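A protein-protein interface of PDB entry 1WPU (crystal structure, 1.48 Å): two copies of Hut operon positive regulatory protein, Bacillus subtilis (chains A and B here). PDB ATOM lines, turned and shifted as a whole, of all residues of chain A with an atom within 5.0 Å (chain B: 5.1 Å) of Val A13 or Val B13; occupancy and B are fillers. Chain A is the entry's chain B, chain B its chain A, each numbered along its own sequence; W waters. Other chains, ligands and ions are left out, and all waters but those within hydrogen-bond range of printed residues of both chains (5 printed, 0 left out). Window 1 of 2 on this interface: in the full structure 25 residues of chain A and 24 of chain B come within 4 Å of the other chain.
Among the printed residues, merely in contact across the chains: Phe A140 with Gly B9, Phe A140 with Val B13, Phe A140 with Arg B10, Leu A17 with Val B13, Gly A9 with Phe B140, Val A13 with Phe B140, Arg A10 with Phe B140, Val A13 with Leu B17, Phe A140 with Val B142, Val A142 with Phe B140, Leu A14 with Leu B17 and Val A13 with Val B13.
Water W3 lies within hydrogen-bond range of the backbone carbonyl oxygen (O) of Phe B140 and the backbone NH (N) of Val A142.
Water W5 lies within hydrogen-bond range of O of Phe A140 (2.9 Å) and N of Val B142 (2.9 Å).
Water W1 bridges O of Val A142 and N of Phe B140.
Water W2 lies within hydrogen-bond range of the backbone carbonyl oxygen of Val B142 (2.9 Å) and the backbone NH of Phe A140 (3.0 Å).
Water W4 lies within hydrogen-bond range of O of Leu B17 (3.4 Å) and NE of Arg A10 (3.5 Å).
Printed residues of chain B that touch a printed residue of chain A: Gly B9, Arg B10, Val B13, Leu B17, Phe B140 and Val B142.
Hydrophobic or aromatic side chains of chain A that line the printed part of chain B: Val A13, Leu A14, Leu A17, Phe A140 and Val A142.
The guanidinium group (NE) of Arg B10 is in hydrogen-bond range of the backbone carbonyl oxygen (O) of Leu A17, at 3.1 Å.
The backbone carbonyl oxygen (O) of Leu B17 is in hydrogen-bond range of the guanidinium group (NE) of Arg A10, 3.0 Å away.
Of chain B, only Val B13 (3.9 Å), Leu B17 (3.7 Å) and Phe B140 (3.6 Å) come within 4 Å of Val A13.
Of chain A, only Val A13, Leu A17 and Phe A140 come within 4 Å of Val B13.
Of the printed residues of chain A, Gly B9 touches Phe A140.
Printed residues of chain B within 4 Å of Phe A140: Gly B9, Arg B10, Val B13 and Val B142.
Of the printed residues of chain B, Arg A10 touches Leu B17 (3.0 Å) and Phe B140 (3.6 Å).
Of the printed residues of chain A, Val B142 touches Phe A140 (3.7 Å).
Leu A16 touches none of the printed residues of chain B.
Ile B8 touches none of the printed residues of chain A.
The nearest printed residue of chain B that does not touch Val A13 is Leu B14 (6.7 Å).
The backbone carbonyl oxygen (O) of Gly B9 sits at hydrogen-bond distance from the side-chain hydroxyl (OG) of Ser B12, at 2.7 Å.
OG of Ser A12 sits at hydrogen-bond distance from O of Gly A9 (2.8 Å).
Arg A10 touches Leu B17, and with the chains exchanged Leu A17 touches Arg B10.
Val B13 touches its own counterpart, Val A13.
Val A13 touches Leu B17, and with the chains exchanged Leu A17 touches Val B13.
Val A13 touches Phe B140, and with the chains exchanged Phe A140 touches Val B13.
Positions printed for both chains: 9, 10, 11, 12, 13, 14, 15, 16, 17, 123, 140 and 142.
Of the 14 pairs that touch across the chains among the printed residues, 13 have their exchanged pair printed and touching as well.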
ATOM      1  N   GLY A   9       7.760  -2.504 -16.233  1.00  0.00           N
ATOM      2  CA  GLY A   9       7.661  -3.775 -15.535  1.00  0.00           C
ATOM      3  C   GLY A   9       6.613  -4.692 -16.149  1.00  0.00           C
ATOM      4  O   GLY A   9       6.910  -5.826 -16.529  1.00  0.00           O
ATOM      5  N   ARG A  10       5.385  -4.195 -16.243  1.00  0.00           N
ATOM      6  CA  ARG A  10       4.280  -4.954 -16.819  1.00  0.00           C
ATOM      7  C   ARG A  10       4.580  -5.388 -18.254  1.00  0.00           C
ATOM      8  O   ARG A  10       4.267  -6.513 -18.645  1.00  0.00           O
ATOM      9  CB  ARG A  10       2.999  -4.113 -16.776  1.00  0.00           C
ATOM     10  CG  ARG A  10       1.791  -4.764 -17.431  1.00  0.00           C
ATOM     11  CD  ARG A  10       0.513  -3.985 -17.145  1.00  0.00           C
ATOM     12  NE  ARG A  10      -0.630  -4.536 -17.869  1.00  0.00           N
ATOM     13  CZ  ARG A  10      -0.835  -4.376 -19.173  1.00  0.00           C
ATOM     14  NH1 ARG A  10       0.025  -3.676 -19.902  1.00  0.00           N
ATOM     15  NH2 ARG A  10      -1.897  -4.923 -19.750  1.00  0.00           N
ATOM     16  N   LEU A  11       5.188  -4.502 -19.037  1.00  0.00           N
ATOM     17  CA  LEU A  11       5.517  -4.822 -20.422  1.00  0.00           C
ATOM     18  C   LEU A  11       6.559  -5.931 -20.529  1.00  0.00           C
ATOM     19  O   LEU A  11       6.447  -6.817 -21.378  1.00  0.00           O
ATOM     20  CB  LEU A  11       6.024  -3.575 -21.159  1.00  0.00           C
ATOM     21  CG  LEU A  11       4.991  -2.485 -21.454  1.00  0.00           C
ATOM     22  CD1 LEU A  11       5.687  -1.280 -22.065  1.00  0.00           C
ATOM     23  CD2 LEU A  11       3.920  -3.026 -22.399  1.00  0.00           C
ATOM     24  N   SER A  12       7.571  -5.888 -19.668  1.00  0.00           N
ATOM     25  CA  SER A  12       8.617  -6.903 -19.707  1.00  0.00           C
ATOM     26  C   SER A  12       8.054  -8.275 -19.353  1.00  0.00           C
ATOM     27  O   SER A  12       8.444  -9.283 -19.943  1.00  0.00           O
ATOM     28  CB  SER A  12       9.760  -6.543 -18.747  1.00  0.00           C
ATOM     29  OG  SER A  12       9.380  -6.694 -17.391  1.00  0.00           O
ATOM     30  N   VAL A  13       7.127  -8.306 -18.398  1.00  0.00           N
ATOM     31  CA  VAL A  13       6.514  -9.552 -17.956  1.00  0.00           C
ATOM     32  C   VAL A  13       5.580 -10.145 -19.004  1.00  0.00           C
ATOM     33  O   VAL A  13       5.590 -11.353 -19.228  1.00  0.00           O
ATOM     34  CB  VAL A  13       5.735  -9.348 -16.631  1.00  0.00           C
ATOM     35  CG1 VAL A  13       4.956 -10.612 -16.274  1.00  0.00           C
ATOM     36  CG2 VAL A  13       6.709  -9.009 -15.512  1.00  0.00           C
ATOM     37  N   LEU A  14       4.776  -9.299 -19.642  1.00  0.00           N
ATOM     38  CA  LEU A  14       3.855  -9.768 -20.670  1.00  0.00           C
ATOM     39  C   LEU A  14       4.632 -10.326 -21.854  1.00  0.00           C
ATOM     40  O   LEU A  14       4.177 -11.254 -22.516  1.00  0.00           O
ATOM     41  CB  LEU A  14       2.941  -8.633 -21.136  1.00  0.00           C
ATOM     42  CG  LEU A  14       1.907  -8.140 -20.119  1.00  0.00           C
ATOM     43  CD2 LEU A  14       0.985  -9.285 -19.714  1.00  0.00           C
ATOM     44  N   LEU A  15       5.806  -9.758 -22.117  1.00  0.00           N
ATOM     45  CA  LEU A  15       6.643 -10.227 -23.216  1.00  0.00           C
ATOM     46  C   LEU A  15       7.205 -11.598 -22.859  1.00  0.00           C
ATOM     47  O   LEU A  15       7.165 -12.531 -23.661  1.00  0.00           O
ATOM     48  CB  LEU A  15       7.797  -9.247 -23.469  1.00  0.00           C
ATOM     49  CG  LEU A  15       8.836  -9.687 -24.509  1.00  0.00           C
ATOM     50  CD1 LEU A  15       8.170  -9.840 -25.870  1.00  0.00           C
ATOM     51  CD2 LEU A  15       9.965  -8.667 -24.575  1.00  0.00           C
ATOM     52  N   LEU A  16       7.719 -11.718 -21.640  1.00  0.00           N
ATOM     53  CA  LEU A  16       8.304 -12.969 -21.180  1.00  0.00           C
ATOM     54  C   LEU A  16       7.282 -14.097 -21.064  1.00  0.00           C
ATOM     55  O   LEU A  16       7.589 -15.250 -21.368  1.00  0.00           O
ATOM     56  CB  LEU A  16       8.991 -12.760 -19.825  1.00  0.00           C
ATOM     57  CG  LEU A  16       9.814 -13.936 -19.287  1.00  0.00           C
ATOM     58  CD1 LEU A  16      11.009 -14.183 -20.199  1.00  0.00           C
ATOM     59  N   LEU A  17       6.067 -13.765 -20.639  1.00  0.00           N
ATOM     60  CA  LEU A  17       5.025 -14.772 -20.466  1.00  0.00           C
ATOM     61  C   LEU A  17       4.217 -15.116 -21.713  1.00  0.00           C
ATOM     62  O   LEU A  17       3.123 -15.670 -21.613  1.00  0.00           O
ATOM     63  CB  LEU A  17       4.074 -14.353 -19.343  1.00  0.00           C
ATOM     64  CG  LEU A  17       4.595 -14.418 -17.908  1.00  0.00           C
ATOM     65  CD1 LEU A  17       3.509 -13.948 -16.950  1.00  0.00           C
ATOM     66  CD2 LEU A  17       5.017 -15.843 -17.581  1.00  0.00           C
ATOM     67  N   SER A 123      13.206  -9.203 -15.942  1.00  0.00           N
ATOM     68  CA  SER A 123      12.130 -10.090 -15.525  1.00  0.00           C
ATOM     69  C   SER A 123      12.497 -11.535 -15.789  1.00  0.00           C
ATOM     70  O   SER A 123      13.043 -11.871 -16.842  1.00  0.00           O
ATOM     71  CB  SER A 123      10.830  -9.721 -16.235  1.00  0.00           C
ATOM     72  OG  SER A 123      10.449  -8.404 -15.876  1.00  0.00           O
ATOM     73  N   PHE A 140       9.130 -16.586 -10.284  1.00  0.00           N
ATOM     74  CA  PHE A 140       9.109 -15.297 -10.979  1.00  0.00           C
ATOM     75  C   PHE A 140       9.954 -14.280 -10.231  1.00  0.00           C
ATOM     76  O   PHE A 140      10.122 -14.371  -9.015  1.00  0.00           O
ATOM     77  CB  PHE A 140       7.708 -14.677 -11.012  1.00  0.00           C
ATOM     78  CG  PHE A 140       6.694 -15.418 -11.823  1.00  0.00           C
ATOM     79  CD1 PHE A 140       6.148 -16.613 -11.371  1.00  0.00           C
ATOM     80  CD2 PHE A 140       6.192 -14.848 -12.991  1.00  0.00           C
ATOM     81  CE1 PHE A 140       5.105 -17.227 -12.068  1.00  0.00           C
ATOM     82  CE2 PHE A 140       5.154 -15.450 -13.691  1.00  0.00           C
ATOM     83  CZ  PHE A 140       4.609 -16.641 -13.227  1.00  0.00           C
ATOM     84  N   VAL A 142      11.139  -9.821 -10.690  1.00  0.00           N
ATOM     85  CA  VAL A 142      11.241  -8.589 -11.460  1.00  0.00           C
ATOM     86  C   VAL A 142      12.054  -7.569 -10.675  1.00  0.00           C
ATOM     87  O   VAL A 142      11.786  -7.325  -9.494  1.00  0.00           O
ATOM     88  CB  VAL A 142       9.852  -7.982 -11.774  1.00  0.00           C
ATOM     89  CG1 VAL A 142      10.024  -6.654 -12.529  1.00  0.00           C
ATOM     90  CG2 VAL A 142       9.041  -8.953 -12.615  1.00  0.00           C
ATOM     91  N   ILE B   8      -0.294 -22.699 -12.899  1.00  0.00           N
ATOM     92  CA  ILE B   8      -0.891 -21.822 -11.899  1.00  0.00           C
ATOM     93  C   ILE B   8      -0.218 -20.461 -11.717  1.00  0.00           C
ATOM     94  O   ILE B   8      -0.901 -19.448 -11.564  1.00  0.00           O
ATOM     95  CB  ILE B   8      -0.977 -22.564 -10.540  1.00  0.00           C
ATOM     96  CG1 ILE B   8      -1.877 -21.795  -9.573  1.00  0.00           C
ATOM     97  CG2 ILE B   8       0.419 -22.767  -9.958  1.00  0.00           C
ATOM     98  CD1 ILE B   8      -2.136 -22.539  -8.274  1.00  0.00           C
ATOM     99  N   GLY B   9       1.111 -20.436 -11.728  1.00  0.00           N
ATOM    100  CA  GLY B   9       1.822 -19.179 -11.569  1.00  0.00           C
ATOM    101  C   GLY B   9       1.571 -18.240 -12.736  1.00  0.00           C
ATOM    102  O   GLY B   9       1.130 -17.104 -12.553  1.00  0.00           O
ATOM    103  N   ARG B  10       1.852 -18.725 -13.940  1.00  0.00           N
ATOM    104  CA  ARG B  10       1.653 -17.946 -15.156  1.00  0.00           C
ATOM    105  C   ARG B  10       0.204 -17.486 -15.299  1.00  0.00           C
ATOM    106  O   ARG B  10      -0.056 -16.347 -15.685  1.00  0.00           O
ATOM    107  CB  ARG B  10       2.063 -18.781 -16.373  1.00  0.00           C
ATOM    108  CG  ARG B  10       1.814 -18.111 -17.714  1.00  0.00           C
ATOM    109  CD  ARG B  10       2.510 -18.873 -18.834  1.00  0.00           C
ATOM    110  NE  ARG B  10       2.218 -18.306 -20.148  1.00  0.00           N
ATOM    111  CZ  ARG B  10       1.045 -18.412 -20.762  1.00  0.00           C
ATOM    112  NH1 ARG B  10       0.049 -19.069 -20.184  1.00  0.00           N
ATOM    113  NH2 ARG B  10       0.864 -17.855 -21.951  1.00  0.00           N
ATOM    114  N   LEU B  11      -0.738 -18.371 -14.987  1.00  0.00           N
ATOM    115  CA  LEU B  11      -2.155 -18.034 -15.087  1.00  0.00           C
ATOM    116  C   LEU B  11      -2.555 -16.942 -14.098  1.00  0.00           C
ATOM    117  O   LEU B  11      -3.329 -16.043 -14.435  1.00  0.00           O
ATOM    118  CB  LEU B  11      -3.021 -19.278 -14.860  1.00  0.00           C
ATOM    119  CG  LEU B  11      -2.998 -20.353 -15.950  1.00  0.00           C
ATOM    120  CD1 LEU B  11      -3.837 -21.542 -15.510  1.00  0.00           C
ATOM    121  CD2 LEU B  11      -3.533 -19.777 -17.258  1.00  0.00           C
ATOM    122  N   SER B  12      -2.030 -17.014 -12.878  1.00  0.00           N
ATOM    123  CA  SER B  12      -2.369 -16.020 -11.867  1.00  0.00           C
ATOM    124  C   SER B  12      -1.830 -14.646 -12.252  1.00  0.00           C
ATOM    125  O   SER B  12      -2.494 -13.633 -12.042  1.00  0.00           O
ATOM    126  CB  SER B  12      -1.818 -16.433 -10.494  1.00  0.00           C
ATOM    127  OG  SER B  12      -0.408 -16.309 -10.431  1.00  0.00           O
ATOM    128  N   VAL B  13      -0.628 -14.621 -12.823  1.00  0.00           N
ATOM    129  CA  VAL B  13       0.001 -13.371 -13.232  1.00  0.00           C
ATOM    130  C   VAL B  13      -0.717 -12.743 -14.419  1.00  0.00           C
ATOM    131  O   VAL B  13      -0.906 -11.528 -14.463  1.00  0.00           O
ATOM    132  CB  VAL B  13       1.493 -13.591 -13.585  1.00  0.00           C
ATOM    133  CG1 VAL B  13       2.092 -12.311 -14.163  1.00  0.00           C
ATOM    134  CG2 VAL B  13       2.259 -14.003 -12.331  1.00  0.00           C
ATOM    135  N   LEU B  14      -1.114 -13.571 -15.381  1.00  0.00           N
ATOM    136  CA  LEU B  14      -1.824 -13.078 -16.554  1.00  0.00           C
ATOM    137  C   LEU B  14      -3.162 -12.472 -16.153  1.00  0.00           C
ATOM    138  O   LEU B  14      -3.588 -11.468 -16.721  1.00  0.00           O
ATOM    139  CB  LEU B  14      -2.041 -14.213 -17.556  1.00  0.00           C
ATOM    140  CG  LEU B  14      -0.875 -14.438 -18.521  1.00  0.00           C
ATOM    141  CD2 LEU B  14      -0.784 -13.236 -19.453  1.00  0.00           C
ATOM    142  N   LEU B  15      -3.819 -13.084 -15.172  1.00  0.00           N
ATOM    143  CA  LEU B  15      -5.102 -12.586 -14.693  1.00  0.00           C
ATOM    144  C   LEU B  15      -4.890 -11.233 -14.031  1.00  0.00           C
ATOM    145  O   LEU B  15      -5.668 -10.299 -14.223  1.00  0.00           O
ATOM    146  CB  LEU B  15      -5.708 -13.563 -13.679  1.00  0.00           C
ATOM    147  CG  LEU B  15      -7.004 -13.114 -12.995  1.00  0.00           C
ATOM    148  CD1 LEU B  15      -8.095 -12.909 -14.038  1.00  0.00           C
ATOM    149  CD2 LEU B  15      -7.429 -14.157 -11.970  1.00  0.00           C
ATOM    150  N   LEU B  16      -3.815 -11.131 -13.259  1.00  0.00           N
ATOM    151  CA  LEU B  16      -3.494  -9.906 -12.542  1.00  0.00           C
ATOM    152  C   LEU B  16      -3.126  -8.731 -13.447  1.00  0.00           C
ATOM    153  O   LEU B  16      -3.469  -7.585 -13.151  1.00  0.00           O
ATOM    154  CB  LEU B  16      -2.350 -10.176 -11.557  1.00  0.00           C
ATOM    155  CG  LEU B  16      -2.038  -9.099 -10.515  1.00  0.00           C
ATOM    156  CD1 LEU B  16      -3.245  -8.900  -9.606  1.00  0.00           C
ATOM    157  N   LEU B  17      -2.442  -9.011 -14.553  1.00  0.00           N
ATOM    158  CA  LEU B  17      -2.011  -7.955 -15.466  1.00  0.00           C
ATOM    159  C   LEU B  17      -3.003  -7.527 -16.544  1.00  0.00           C
ATOM    160  O   LEU B  17      -2.674  -6.691 -17.385  1.00  0.00           O
ATOM    161  CB  LEU B  17      -0.688  -8.352 -16.130  1.00  0.00           C
ATOM    162  CG  LEU B  17       0.515  -8.469 -15.190  1.00  0.00           C
ATOM    163  CD1 LEU B  17       1.745  -8.876 -15.984  1.00  0.00           C
ATOM    164  CD2 LEU B  17       0.748  -7.135 -14.486  1.00  0.00           C
ATOM    165  N   SER B 123      -0.151 -13.883  -6.277  1.00  0.00           N
ATOM    166  CA  SER B 123       0.580 -12.984  -7.154  1.00  0.00           C
ATOM    167  C   SER B 123       0.241 -11.545  -6.836  1.00  0.00           C
ATOM    168  O   SER B 123      -0.916 -11.208  -6.580  1.00  0.00           O
ATOM    169  CB  SER B 123       0.273 -13.304  -8.615  1.00  0.00           C
ATOM    170  OG  SER B 123       0.671 -14.633  -8.899  1.00  0.00           O
ATOM    171  N   PHE B 140       6.617  -6.577  -8.270  1.00  0.00           N
ATOM    172  CA  PHE B 140       5.941  -7.847  -8.532  1.00  0.00           C
ATOM    173  C   PHE B 140       6.368  -8.892  -7.517  1.00  0.00           C
ATOM    174  O   PHE B 140       7.478  -8.840  -6.986  1.00  0.00           O
ATOM    175  CB  PHE B 140       6.337  -8.444  -9.887  1.00  0.00           C
ATOM    176  CG  PHE B 140       5.851  -7.694 -11.085  1.00  0.00           C
ATOM    177  CD1 PHE B 140       6.442  -6.496 -11.471  1.00  0.00           C
ATOM    178  CD2 PHE B 140       4.873  -8.255 -11.904  1.00  0.00           C
ATOM    179  CE1 PHE B 140       6.071  -5.871 -12.663  1.00  0.00           C
ATOM    180  CE2 PHE B 140       4.498  -7.640 -13.092  1.00  0.00           C
ATOM    181  CZ  PHE B 140       5.099  -6.449 -13.473  1.00  0.00           C
ATOM    182  N   VAL B 142       5.481 -13.347  -6.645  1.00  0.00           N
ATOM    183  CA  VAL B 142       4.688 -14.561  -6.811  1.00  0.00           C
ATOM    184  C   VAL B 142       5.168 -15.616  -5.823  1.00  0.00           C
ATOM    185  O   VAL B 142       6.372 -15.886  -5.722  1.00  0.00           O
ATOM    186  CB  VAL B 142       4.798 -15.141  -8.243  1.00  0.00           C
ATOM    187  CG1 VAL B 142       3.942 -16.412  -8.358  1.00  0.00           C
ATOM    188  CG2 VAL B 142       4.341 -14.105  -9.262  1.00  0.00           C
HETATM  189  O   HOH W   1       9.620  -6.511  -7.782  1.00  0.00           O
HETATM  190  O   HOH W   2       8.665 -16.745  -7.277  1.00  0.00           O
HETATM  191  O   HOH W   3       9.552 -10.248  -8.226  1.00  0.00           O
HETATM  192  O   HOH W   4      -2.219  -4.507 -14.806  1.00  0.00           O
HETATM  193  O   HOH W   5       8.254 -12.987  -7.342  1.00  0.00           O
